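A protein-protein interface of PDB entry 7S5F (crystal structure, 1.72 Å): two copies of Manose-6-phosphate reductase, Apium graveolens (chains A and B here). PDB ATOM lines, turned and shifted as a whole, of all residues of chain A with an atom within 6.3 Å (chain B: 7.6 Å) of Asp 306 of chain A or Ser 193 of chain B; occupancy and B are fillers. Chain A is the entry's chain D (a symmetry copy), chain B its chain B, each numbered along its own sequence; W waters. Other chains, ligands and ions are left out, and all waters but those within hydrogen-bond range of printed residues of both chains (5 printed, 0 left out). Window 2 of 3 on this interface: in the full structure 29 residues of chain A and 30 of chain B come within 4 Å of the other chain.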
ATOM      1  N   THR A 298      -9.713  28.985  28.154  1.00  0.00           N
ATOM      2  CA  THR A 298      -8.878  27.834  28.462  1.00  0.00           C
ATOM      3  C   THR A 298      -7.507  28.313  28.919  1.00  0.00           C
ATOM      4  O   THR A 298      -6.916  29.200  28.275  1.00  0.00           O
ATOM      5  CB  THR A 298      -8.738  26.859  27.284  1.00  0.00           C
ATOM      6  OG1 THR A 298      -7.853  25.791  27.649  1.00  0.00           O
ATOM      7  CG2 THR A 298      -8.254  27.557  26.026  1.00  0.00           C
ATOM      8  N   PRO A 299      -6.990  27.764  30.020  1.00  0.00           N
ATOM      9  CA  PRO A 299      -5.634  28.091  30.459  1.00  0.00           C
ATOM     10  C   PRO A 299      -4.543  27.284  29.775  1.00  0.00           C
ATOM     11  O   PRO A 299      -3.400  27.324  30.238  1.00  0.00           O
ATOM     12  CB  PRO A 299      -5.691  27.753  31.955  1.00  0.00           C
ATOM     13  CG  PRO A 299      -6.582  26.547  31.994  1.00  0.00           C
ATOM     14  CD  PRO A 299      -7.662  26.847  30.958  1.00  0.00           C
ATOM     15  N   ALA A 300      -4.882  26.552  28.708  1.00  0.00           N
ATOM     16  CA  ALA A 300      -3.935  25.633  28.081  1.00  0.00           C
ATOM     17  C   ALA A 300      -2.642  26.337  27.684  1.00  0.00           C
ATOM     18  O   ALA A 300      -1.548  25.829  27.946  1.00  0.00           O
ATOM     19  CB  ALA A 300      -4.583  24.970  26.862  1.00  0.00           C
ATOM     20  N   LYS A 301      -2.744  27.519  27.074  1.00  0.00           N
ATOM     21  CA  LYS A 301      -1.534  28.196  26.618  1.00  0.00           C
ATOM     22  C   LYS A 301      -0.724  28.726  27.793  1.00  0.00           C
ATOM     23  O   LYS A 301       0.504  28.585  27.821  1.00  0.00           O
ATOM     24  CB  LYS A 301      -1.890  29.328  25.654  1.00  0.00           C
ATOM     25  CG  LYS A 301      -0.681  29.911  24.949  1.00  0.00           C
ATOM     26  CD  LYS A 301      -1.079  30.784  23.771  1.00  0.00           C
ATOM     27  CE  LYS A 301      -0.263  32.069  23.752  1.00  0.00           C
ATOM     28  NZ  LYS A 301       0.284  32.362  22.401  1.00  0.00           N
ATOM     29  N   GLY A 304       0.800  25.679  29.623  1.00  0.00           N
ATOM     30  CA  GLY A 304       1.554  24.735  28.828  1.00  0.00           C
ATOM     31  C   GLY A 304       1.023  23.324  28.902  1.00  0.00           C
ATOM     32  O   GLY A 304       1.761  22.375  28.618  1.00  0.00           O
ATOM     33  N   ILE A 305      -0.236  23.158  29.313  1.00  0.00           N
ATOM     34  CA  ILE A 305      -0.898  21.857  29.350  1.00  0.00           C
ATOM     35  C   ILE A 305      -2.348  22.076  28.962  1.00  0.00           C
ATOM     36  O   ILE A 305      -3.024  22.918  29.558  1.00  0.00           O
ATOM     37  CB  ILE A 305      -0.867  21.195  30.744  1.00  0.00           C
ATOM     38  CG1 ILE A 305       0.515  21.196  31.367  1.00  0.00           C
ATOM     39  CG2 ILE A 305      -1.344  19.741  30.649  1.00  0.00           C
ATOM     40  CD1 ILE A 305       0.523  20.600  32.771  1.00  0.00           C
ATOM     41  N   ASP A 306      -2.842  21.315  27.987  1.00  0.00           N
ATOM     42  CA  ASP A 306      -4.269  21.375  27.675  1.00  0.00           C
ATOM     43  C   ASP A 306      -4.998  20.475  28.662  1.00  0.00           C
ATOM     44  O   ASP A 306      -5.091  19.261  28.467  1.00  0.00           O
ATOM     45  CB  ASP A 306      -4.544  20.948  26.238  1.00  0.00           C
ATOM     46  CG  ASP A 306      -6.027  21.042  25.880  1.00  0.00           C
ATOM     47  OD1 ASP A 306      -6.827  21.553  26.700  1.00  0.00           O
ATOM     48  OD2 ASP A 306      -6.400  20.590  24.780  1.00  0.00           O
ATOM     49  N   VAL A 307      -5.520  21.074  29.735  1.00  0.00           N
ATOM     50  CA  VAL A 307      -6.243  20.308  30.744  1.00  0.00           C
ATOM     51  C   VAL A 307      -7.536  19.718  30.211  1.00  0.00           C
ATOM     52  O   VAL A 307      -8.105  18.823  30.846  1.00  0.00           O
ATOM     53  CB  VAL A 307      -6.551  21.172  31.983  1.00  0.00           C
ATOM     54  CG1 VAL A 307      -5.279  21.409  32.800  1.00  0.00           C
ATOM     55  CG2 VAL A 307      -7.196  22.496  31.560  1.00  0.00           C
ATOM     56  N   TYR A 308      -8.014  20.192  29.063  1.00  0.00           N
ATOM     57  CA  TYR A 308      -9.220  19.675  28.435  1.00  0.00           C
ATOM     58  C   TYR A 308      -8.913  18.640  27.363  1.00  0.00           C
ATOM     59  O   TYR A 308      -9.785  18.326  26.546  1.00  0.00           O
ATOM     60  CB  TYR A 308     -10.035  20.829  27.847  1.00  0.00           C
ATOM     61  CG  TYR A 308     -10.439  21.821  28.901  1.00  0.00           C
ATOM     62  CD1 TYR A 308     -11.225  21.429  29.978  1.00  0.00           C
ATOM     63  CD2 TYR A 308     -10.014  23.147  28.842  1.00  0.00           C
ATOM     64  CE1 TYR A 308     -11.590  22.333  30.959  1.00  0.00           C
ATOM     65  CE2 TYR A 308     -10.370  24.060  29.825  1.00  0.00           C
ATOM     66  CZ  TYR A 308     -11.158  23.647  30.877  1.00  0.00           C
ATOM     67  OH  TYR A 308     -11.518  24.553  31.853  1.00  0.00           O
ATOM     68  N   ALA A 309      -7.697  18.099  27.358  1.00  0.00           N
ATOM     69  CA  ALA A 309      -7.278  17.140  26.349  1.00  0.00           C
ATOM     70  C   ALA A 309      -8.065  15.834  26.438  1.00  0.00           C
ATOM     71  O   ALA A 309      -8.212  15.152  25.431  1.00  0.00           O
ATOM     72  CB  ALA A 309      -5.780  16.863  26.472  1.00  0.00           C
ATOM     73  OXT ALA A 309      -8.573  15.432  27.496  1.00  0.00           O
ATOM     74  N   ASP B 163      -9.030  11.945  32.795  1.00  0.00           N
ATOM     75  CA  ASP B 163      -8.413  13.091  32.145  1.00  0.00           C
ATOM     76  C   ASP B 163      -7.267  13.622  33.005  1.00  0.00           C
ATOM     77  O   ASP B 163      -6.859  12.989  33.983  1.00  0.00           O
ATOM     78  CB  ASP B 163      -9.474  14.145  31.850  1.00  0.00           C
ATOM     79  CG  ASP B 163     -10.111  14.708  33.112  1.00  0.00           C
ATOM     80  OD1 ASP B 163      -9.720  14.310  34.231  1.00  0.00           O
ATOM     81  OD2 ASP B 163     -11.044  15.523  32.977  1.00  0.00           O
ATOM     82  N   VAL B 164      -6.729  14.792  32.645  1.00  0.00           N
ATOM     83  CA  VAL B 164      -5.583  15.338  33.380  1.00  0.00           C
ATOM     84  C   VAL B 164      -5.954  15.600  34.837  1.00  0.00           C
ATOM     85  O   VAL B 164      -5.184  15.287  35.753  1.00  0.00           O
ATOM     86  CB  VAL B 164      -5.049  16.612  32.699  1.00  0.00           C
ATOM     87  CG1 VAL B 164      -4.150  17.392  33.664  1.00  0.00           C
ATOM     88  CG2 VAL B 164      -4.285  16.269  31.411  1.00  0.00           C
ATOM     89  N   TYR B 165      -7.137  16.173  35.079  1.00  0.00           N
ATOM     90  CA  TYR B 165      -7.515  16.502  36.449  1.00  0.00           C
ATOM     91  C   TYR B 165      -7.684  15.248  37.290  1.00  0.00           C
ATOM     92  O   TYR B 165      -7.222  15.184  38.437  1.00  0.00           O
ATOM     93  CB  TYR B 165      -8.813  17.301  36.460  1.00  0.00           C
ATOM     94  CG  TYR B 165      -8.735  18.696  35.898  1.00  0.00           C
ATOM     95  CD1 TYR B 165      -7.701  19.551  36.245  1.00  0.00           C
ATOM     96  CD2 TYR B 165      -9.731  19.169  35.050  1.00  0.00           C
ATOM     97  CE1 TYR B 165      -7.648  20.841  35.748  1.00  0.00           C
ATOM     98  CE2 TYR B 165      -9.688  20.457  34.551  1.00  0.00           C
ATOM     99  CZ  TYR B 165      -8.647  21.289  34.906  1.00  0.00           C
ATOM    100  OH  TYR B 165      -8.619  22.566  34.409  1.00  0.00           O
ATOM    101  N   GLN B 190      -5.515  13.021  19.291  1.00  0.00           N
ATOM    102  CA  GLN B 190      -4.152  12.628  19.665  1.00  0.00           C
ATOM    103  C   GLN B 190      -3.793  12.922  21.117  1.00  0.00           C
ATOM    104  O   GLN B 190      -2.914  12.246  21.661  1.00  0.00           O
ATOM    105  CB  GLN B 190      -3.137  13.288  18.719  1.00  0.00           C
ATOM    106  CG  GLN B 190      -3.337  12.832  17.285  1.00  0.00           C
ATOM    107  CD  GLN B 190      -2.275  13.297  16.314  1.00  0.00           C
ATOM    108  OE1 GLN B 190      -1.219  13.798  16.699  1.00  0.00           O
ATOM    109  NE2 GLN B 190      -2.576  13.167  15.027  1.00  0.00           N
ATOM    110  N   ARG B 191      -4.448  13.903  21.747  1.00  0.00           N
ATOM    111  CA  ARG B 191      -4.392  14.111  23.201  1.00  0.00           C
ATOM    112  C   ARG B 191      -2.964  14.174  23.741  1.00  0.00           C
ATOM    113  O   ARG B 191      -2.648  13.579  24.774  1.00  0.00           O
ATOM    114  CB  ARG B 191      -5.187  13.025  23.917  1.00  0.00           C
ATOM    115  CG  ARG B 191      -6.568  12.833  23.327  1.00  0.00           C
ATOM    116  CD  ARG B 191      -7.354  11.845  24.152  1.00  0.00           C
ATOM    117  NE  ARG B 191      -8.001  12.446  25.311  1.00  0.00           N
ATOM    118  CZ  ARG B 191      -8.809  11.779  26.124  1.00  0.00           C
ATOM    119  NH1 ARG B 191      -9.071  10.495  25.930  1.00  0.00           N
ATOM    120  NH2 ARG B 191      -9.371  12.419  27.153  1.00  0.00           N
ATOM    121  N   ASP B 192      -2.105  14.923  23.045  1.00  0.00           N
ATOM    122  CA  ASP B 192      -0.691  14.987  23.411  1.00  0.00           C
ATOM    123  C   ASP B 192      -0.496  15.361  24.879  1.00  0.00           C
ATOM    124  O   ASP B 192       0.329  14.760  25.576  1.00  0.00           O
ATOM    125  CB  ASP B 192       0.025  15.992  22.513  1.00  0.00           C
ATOM    126  CG  ASP B 192       0.376  15.415  21.154  1.00  0.00           C
ATOM    127  OD1 ASP B 192       0.218  14.196  20.952  1.00  0.00           O
ATOM    128  OD2 ASP B 192       0.808  16.190  20.283  1.00  0.00           O
ATOM    129  N   SER B 193      -1.260  16.344  25.372  1.00  0.00           N
ATOM    130  CA  SER B 193      -1.050  16.833  26.733  1.00  0.00           C
ATOM    131  C   SER B 193      -1.323  15.749  27.770  1.00  0.00           C
ATOM    132  O   SER B 193      -0.587  15.619  28.754  1.00  0.00           O
ATOM    133  CB  SER B 193      -1.941  18.047  27.002  1.00  0.00           C
ATOM    134  OG  SER B 193      -1.408  19.225  26.431  1.00  0.00           O
ATOM    135  N   LEU B 194      -2.387  14.974  27.578  1.00  0.00           N
ATOM    136  CA  LEU B 194      -2.738  13.943  28.550  1.00  0.00           C
ATOM    137  C   LEU B 194      -1.741  12.794  28.527  1.00  0.00           C
ATOM    138  O   LEU B 194      -1.355  12.272  29.579  1.00  0.00           O
ATOM    139  CB  LEU B 194      -4.155  13.442  28.269  1.00  0.00           C
ATOM    140  CG  LEU B 194      -4.690  12.325  29.161  1.00  0.00           C
ATOM    141  CD1 LEU B 194      -4.625  12.731  30.635  1.00  0.00           C
ATOM    142  CD2 LEU B 194      -6.130  12.024  28.756  1.00  0.00           C
ATOM    143  N   ILE B 195      -1.317  12.385  27.338  1.00  0.00           N
ATOM    144  CA  ILE B 195      -0.327  11.316  27.233  1.00  0.00           C
ATOM    145  C   ILE B 195       0.992  11.759  27.853  1.00  0.00           C
ATOM    146  O   ILE B 195       1.619  11.021  28.621  1.00  0.00           O
ATOM    147  CB  ILE B 195      -0.160  10.898  25.764  1.00  0.00           C
ATOM    148  CG1 ILE B 195      -1.438  10.198  25.282  1.00  0.00           C
ATOM    149  CG2 ILE B 195       1.076  10.016  25.590  1.00  0.00           C
ATOM    150  CD1 ILE B 195      -1.543  10.060  23.780  1.00  0.00           C
ATOM    151  N   LYS B 196       1.429  12.976  27.524  1.00  0.00           N
ATOM    152  CA  LYS B 196       2.651  13.530  28.107  1.00  0.00           C
ATOM    153  C   LYS B 196       2.584  13.549  29.631  1.00  0.00           C
ATOM    154  O   LYS B 196       3.552  13.190  30.311  1.00  0.00           O
ATOM    155  CB  LYS B 196       2.869  14.940  27.565  1.00  0.00           C
ATOM    156  CG  LYS B 196       4.105  15.674  28.048  1.00  0.00           C
ATOM    157  CD  LYS B 196       4.175  17.035  27.338  1.00  0.00           C
ATOM    158  CE  LYS B 196       5.291  17.910  27.854  1.00  0.00           C
ATOM    159  NZ  LYS B 196       6.638  17.344  27.559  1.00  0.00           N
ATOM    160  N   PHE B 197       1.450  14.000  30.180  1.00  0.00           N
ATOM    161  CA  PHE B 197       1.286  14.079  31.626  1.00  0.00           C
ATOM    162  C   PHE B 197       1.373  12.700  32.261  1.00  0.00           C
ATOM    163  O   PHE B 197       2.070  12.500  33.263  1.00  0.00           O
ATOM    164  CB  PHE B 197      -0.055  14.738  31.948  1.00  0.00           C
ATOM    165  CG  PHE B 197      -0.294  14.937  33.408  1.00  0.00           C
ATOM    166  CD1 PHE B 197       0.355  15.950  34.093  1.00  0.00           C
ATOM    167  CD2 PHE B 197      -1.165  14.113  34.099  1.00  0.00           C
ATOM    168  CE1 PHE B 197       0.134  16.142  35.446  1.00  0.00           C
ATOM    169  CE2 PHE B 197      -1.391  14.294  35.452  1.00  0.00           C
ATOM    170  CZ  PHE B 197      -0.744  15.313  36.131  1.00  0.00           C
ATOM    171  N   CYS B 198       0.688  11.725  31.669  1.00  0.00           N
ATOM    172  CA  CYS B 198       0.681  10.392  32.247  1.00  0.00           C
ATOM    173  C   CYS B 198       2.074   9.786  32.195  1.00  0.00           C
ATOM    174  O   CYS B 198       2.553   9.208  33.177  1.00  0.00           O
ATOM    175  CB  CYS B 198      -0.323   9.532  31.487  1.00  0.00           C
ATOM    176  SG  CYS B 198      -2.027   9.856  31.991  1.00  0.00           S
ATOM    177  N   HIS B 199       2.761   9.948  31.060  1.00  0.00           N
ATOM    178  CA  HIS B 199       4.102   9.402  30.927  1.00  0.00           C
ATOM    179  C   HIS B 199       5.066  10.050  31.909  1.00  0.00           C
ATOM    180  O   HIS B 199       5.965   9.378  32.429  1.00  0.00           O
ATOM    181  CB  HIS B 199       4.581   9.575  29.484  1.00  0.00           C
ATOM    182  CG  HIS B 199       4.005   8.564  28.543  1.00  0.00           C
ATOM    183  ND1 HIS B 199       4.226   8.593  27.182  1.00  0.00           N
ATOM    184  CD2 HIS B 199       3.208   7.494  28.771  1.00  0.00           C
ATOM    185  CE1 HIS B 199       3.594   7.579  26.615  1.00  0.00           C
ATOM    186  NE2 HIS B 199       2.965   6.899  27.557  1.00  0.00           N
ATOM    187  N   ARG B 254       4.385   6.062  19.353  1.00  0.00           N
ATOM    188  CA  ARG B 254       4.124   7.049  20.401  1.00  0.00           C
ATOM    189  C   ARG B 254       4.316   6.472  21.806  1.00  0.00           C
ATOM    190  O   ARG B 254       3.974   7.144  22.790  1.00  0.00           O
ATOM    191  CB  ARG B 254       2.707   7.622  20.268  1.00  0.00           C
ATOM    192  CG  ARG B 254       2.477   8.439  19.003  1.00  0.00           C
ATOM    193  CD  ARG B 254       1.390   9.481  19.206  1.00  0.00           C
ATOM    194  NE  ARG B 254       0.177   8.874  19.735  1.00  0.00           N
ATOM    195  CZ  ARG B 254      -0.842   9.549  20.246  1.00  0.00           C
ATOM    196  NH1 ARG B 254      -1.918   8.928  20.699  1.00  0.00           N
ATOM    197  NH2 ARG B 254      -0.777  10.880  20.309  1.00  0.00           N
ATOM    198  N   GLU B 291      -4.427  15.603  13.517  1.00  0.00           N
ATOM    199  CA  GLU B 291      -5.066  15.981  14.773  1.00  0.00           C
ATOM    200  C   GLU B 291      -6.234  16.922  14.549  1.00  0.00           C
ATOM    201  O   GLU B 291      -6.094  17.972  13.914  1.00  0.00           O
ATOM    202  CB  GLU B 291      -4.007  16.591  15.694  1.00  0.00           C
ATOM    203  CG  GLU B 291      -4.377  17.302  17.022  1.00  0.00           C
ATOM    204  CD  GLU B 291      -5.298  16.544  17.970  1.00  0.00           C
ATOM    205  OE1 GLU B 291      -5.574  15.358  17.784  1.00  0.00           O
ATOM    206  OE2 GLU B 291      -5.640  17.114  19.020  1.00  0.00           O
ATOM    207  N   ASN B 293      -8.672  16.825  17.411  1.00  0.00           N
ATOM    208  CA  ASN B 293      -9.183  16.899  18.783  1.00  0.00           C
ATOM    209  C   ASN B 293     -10.664  16.536  18.829  1.00  0.00           C
ATOM    210  O   ASN B 293     -11.491  17.246  19.410  1.00  0.00           O
ATOM    211  CB  ASN B 293      -8.939  18.284  19.388  1.00  0.00           C
ATOM    212  CG  ASN B 293      -9.139  18.309  20.894  1.00  0.00           C
ATOM    213  OD1 ASN B 293      -9.256  17.269  21.540  1.00  0.00           O
ATOM    214  ND2 ASN B 293      -9.157  19.506  21.459  1.00  0.00           N
HETATM  215  O   HOH W   1      -9.172  20.365  24.228  1.00  0.00           O
HETATM  216  O   HOH W   2     -10.623  17.855  31.573  1.00  0.00           O
HETATM  217  O   HOH W   3      -7.554  16.553  23.155  1.00  0.00           O
HETATM  218  O   HOH W   4      -7.370  16.048  30.172  1.00  0.00           O
HETATM  219  O   HOH W   5     -11.041  23.452  34.254  1.00  0.00           O
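The guanidinium group of Arg 191 of chain B is in salt-bridge range of the chain-end carboxylate of Ala 309 of chain A, at 2.7 Å. N of Asp 306 of chain A lies within hydrogen-bond range of OG of Ser 193 of chain B, at 3.0 Å.
The side-chain carboxylate (OD1) of Asp 163 of chain B lies close to the backbone NH (N) of Tyr 165 of chain B (3.3 Å). O of Ala 300 of chain A is in hydrogen-bond range of N of Ile 305 of chain A, at 3.3 Å. N of Tyr 308 of chain A sits at hydrogen-bond distance from OD1 of Asp 306 of chain A (3.0 Å).
Of the printed residues of chain B, Asp 306 of chain A touches Ser 193 (3.0 Å). Of chain A, only Ile 305 and Asp 306 come within 4 Å of Ser 193 of chain B. Printed residues of chain B within 4 Å of Ala 309 of chain A: Arg 191 (2.7 Å). Of the printed residues of chain A, Tyr 165 of chain B touches Val 307. Asn 293 of chain B touches none of the printed residues of chain A. The nearest residue of chain B that does not touch Asp 306 of chain A is Val 164 of chain B (4.3 Å). The nearest printed residue of chain A that does not touch Arg 191 of chain B is Tyr 308 of chain A (6.0 Å).
Among the printed residues, 4 pairs touch across the chains.
Ser 193 of chain B touches Ile 305 of chain A. Tyr 165 of chain B touches Val 307 of chain A.
Water W3 lies within hydrogen-bond range of the side-chain amide oxygen (OD1) of Asn 293 of chain B (2.5 Å) and the chain-end carboxylate (O) of Ala 309 of chain A (2.8 Å). Water W5 lies within hydrogen-bond range of the side-chain hydroxyl of Tyr 165 of chain B (2.6 Å) and the side-chain hydroxyl of Tyr 308 of chain A (2.7 Å). Water W2 lies within hydrogen-bond range of the side-chain carboxylate of Asp 163 of chain B (2.8 Å) and the backbone carbonyl oxygen of Val 307 of chain A (2.8 Å). Water W1 lies within hydrogen-bond range of OD2 of Asp 306 of chain A, ND2 of Asn 293 of chain B and O of Tyr 308 of chain A. Water W4 lies within hydrogen-bond range of N of Val 164 of chain B, O of Val 307 of chain A and OXT of Ala 309 of chain A.
No position is printed for both chains. Of the 4 pairs that touch across the chains among the printed residues, none has its exchanged pair printed and touching as well.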
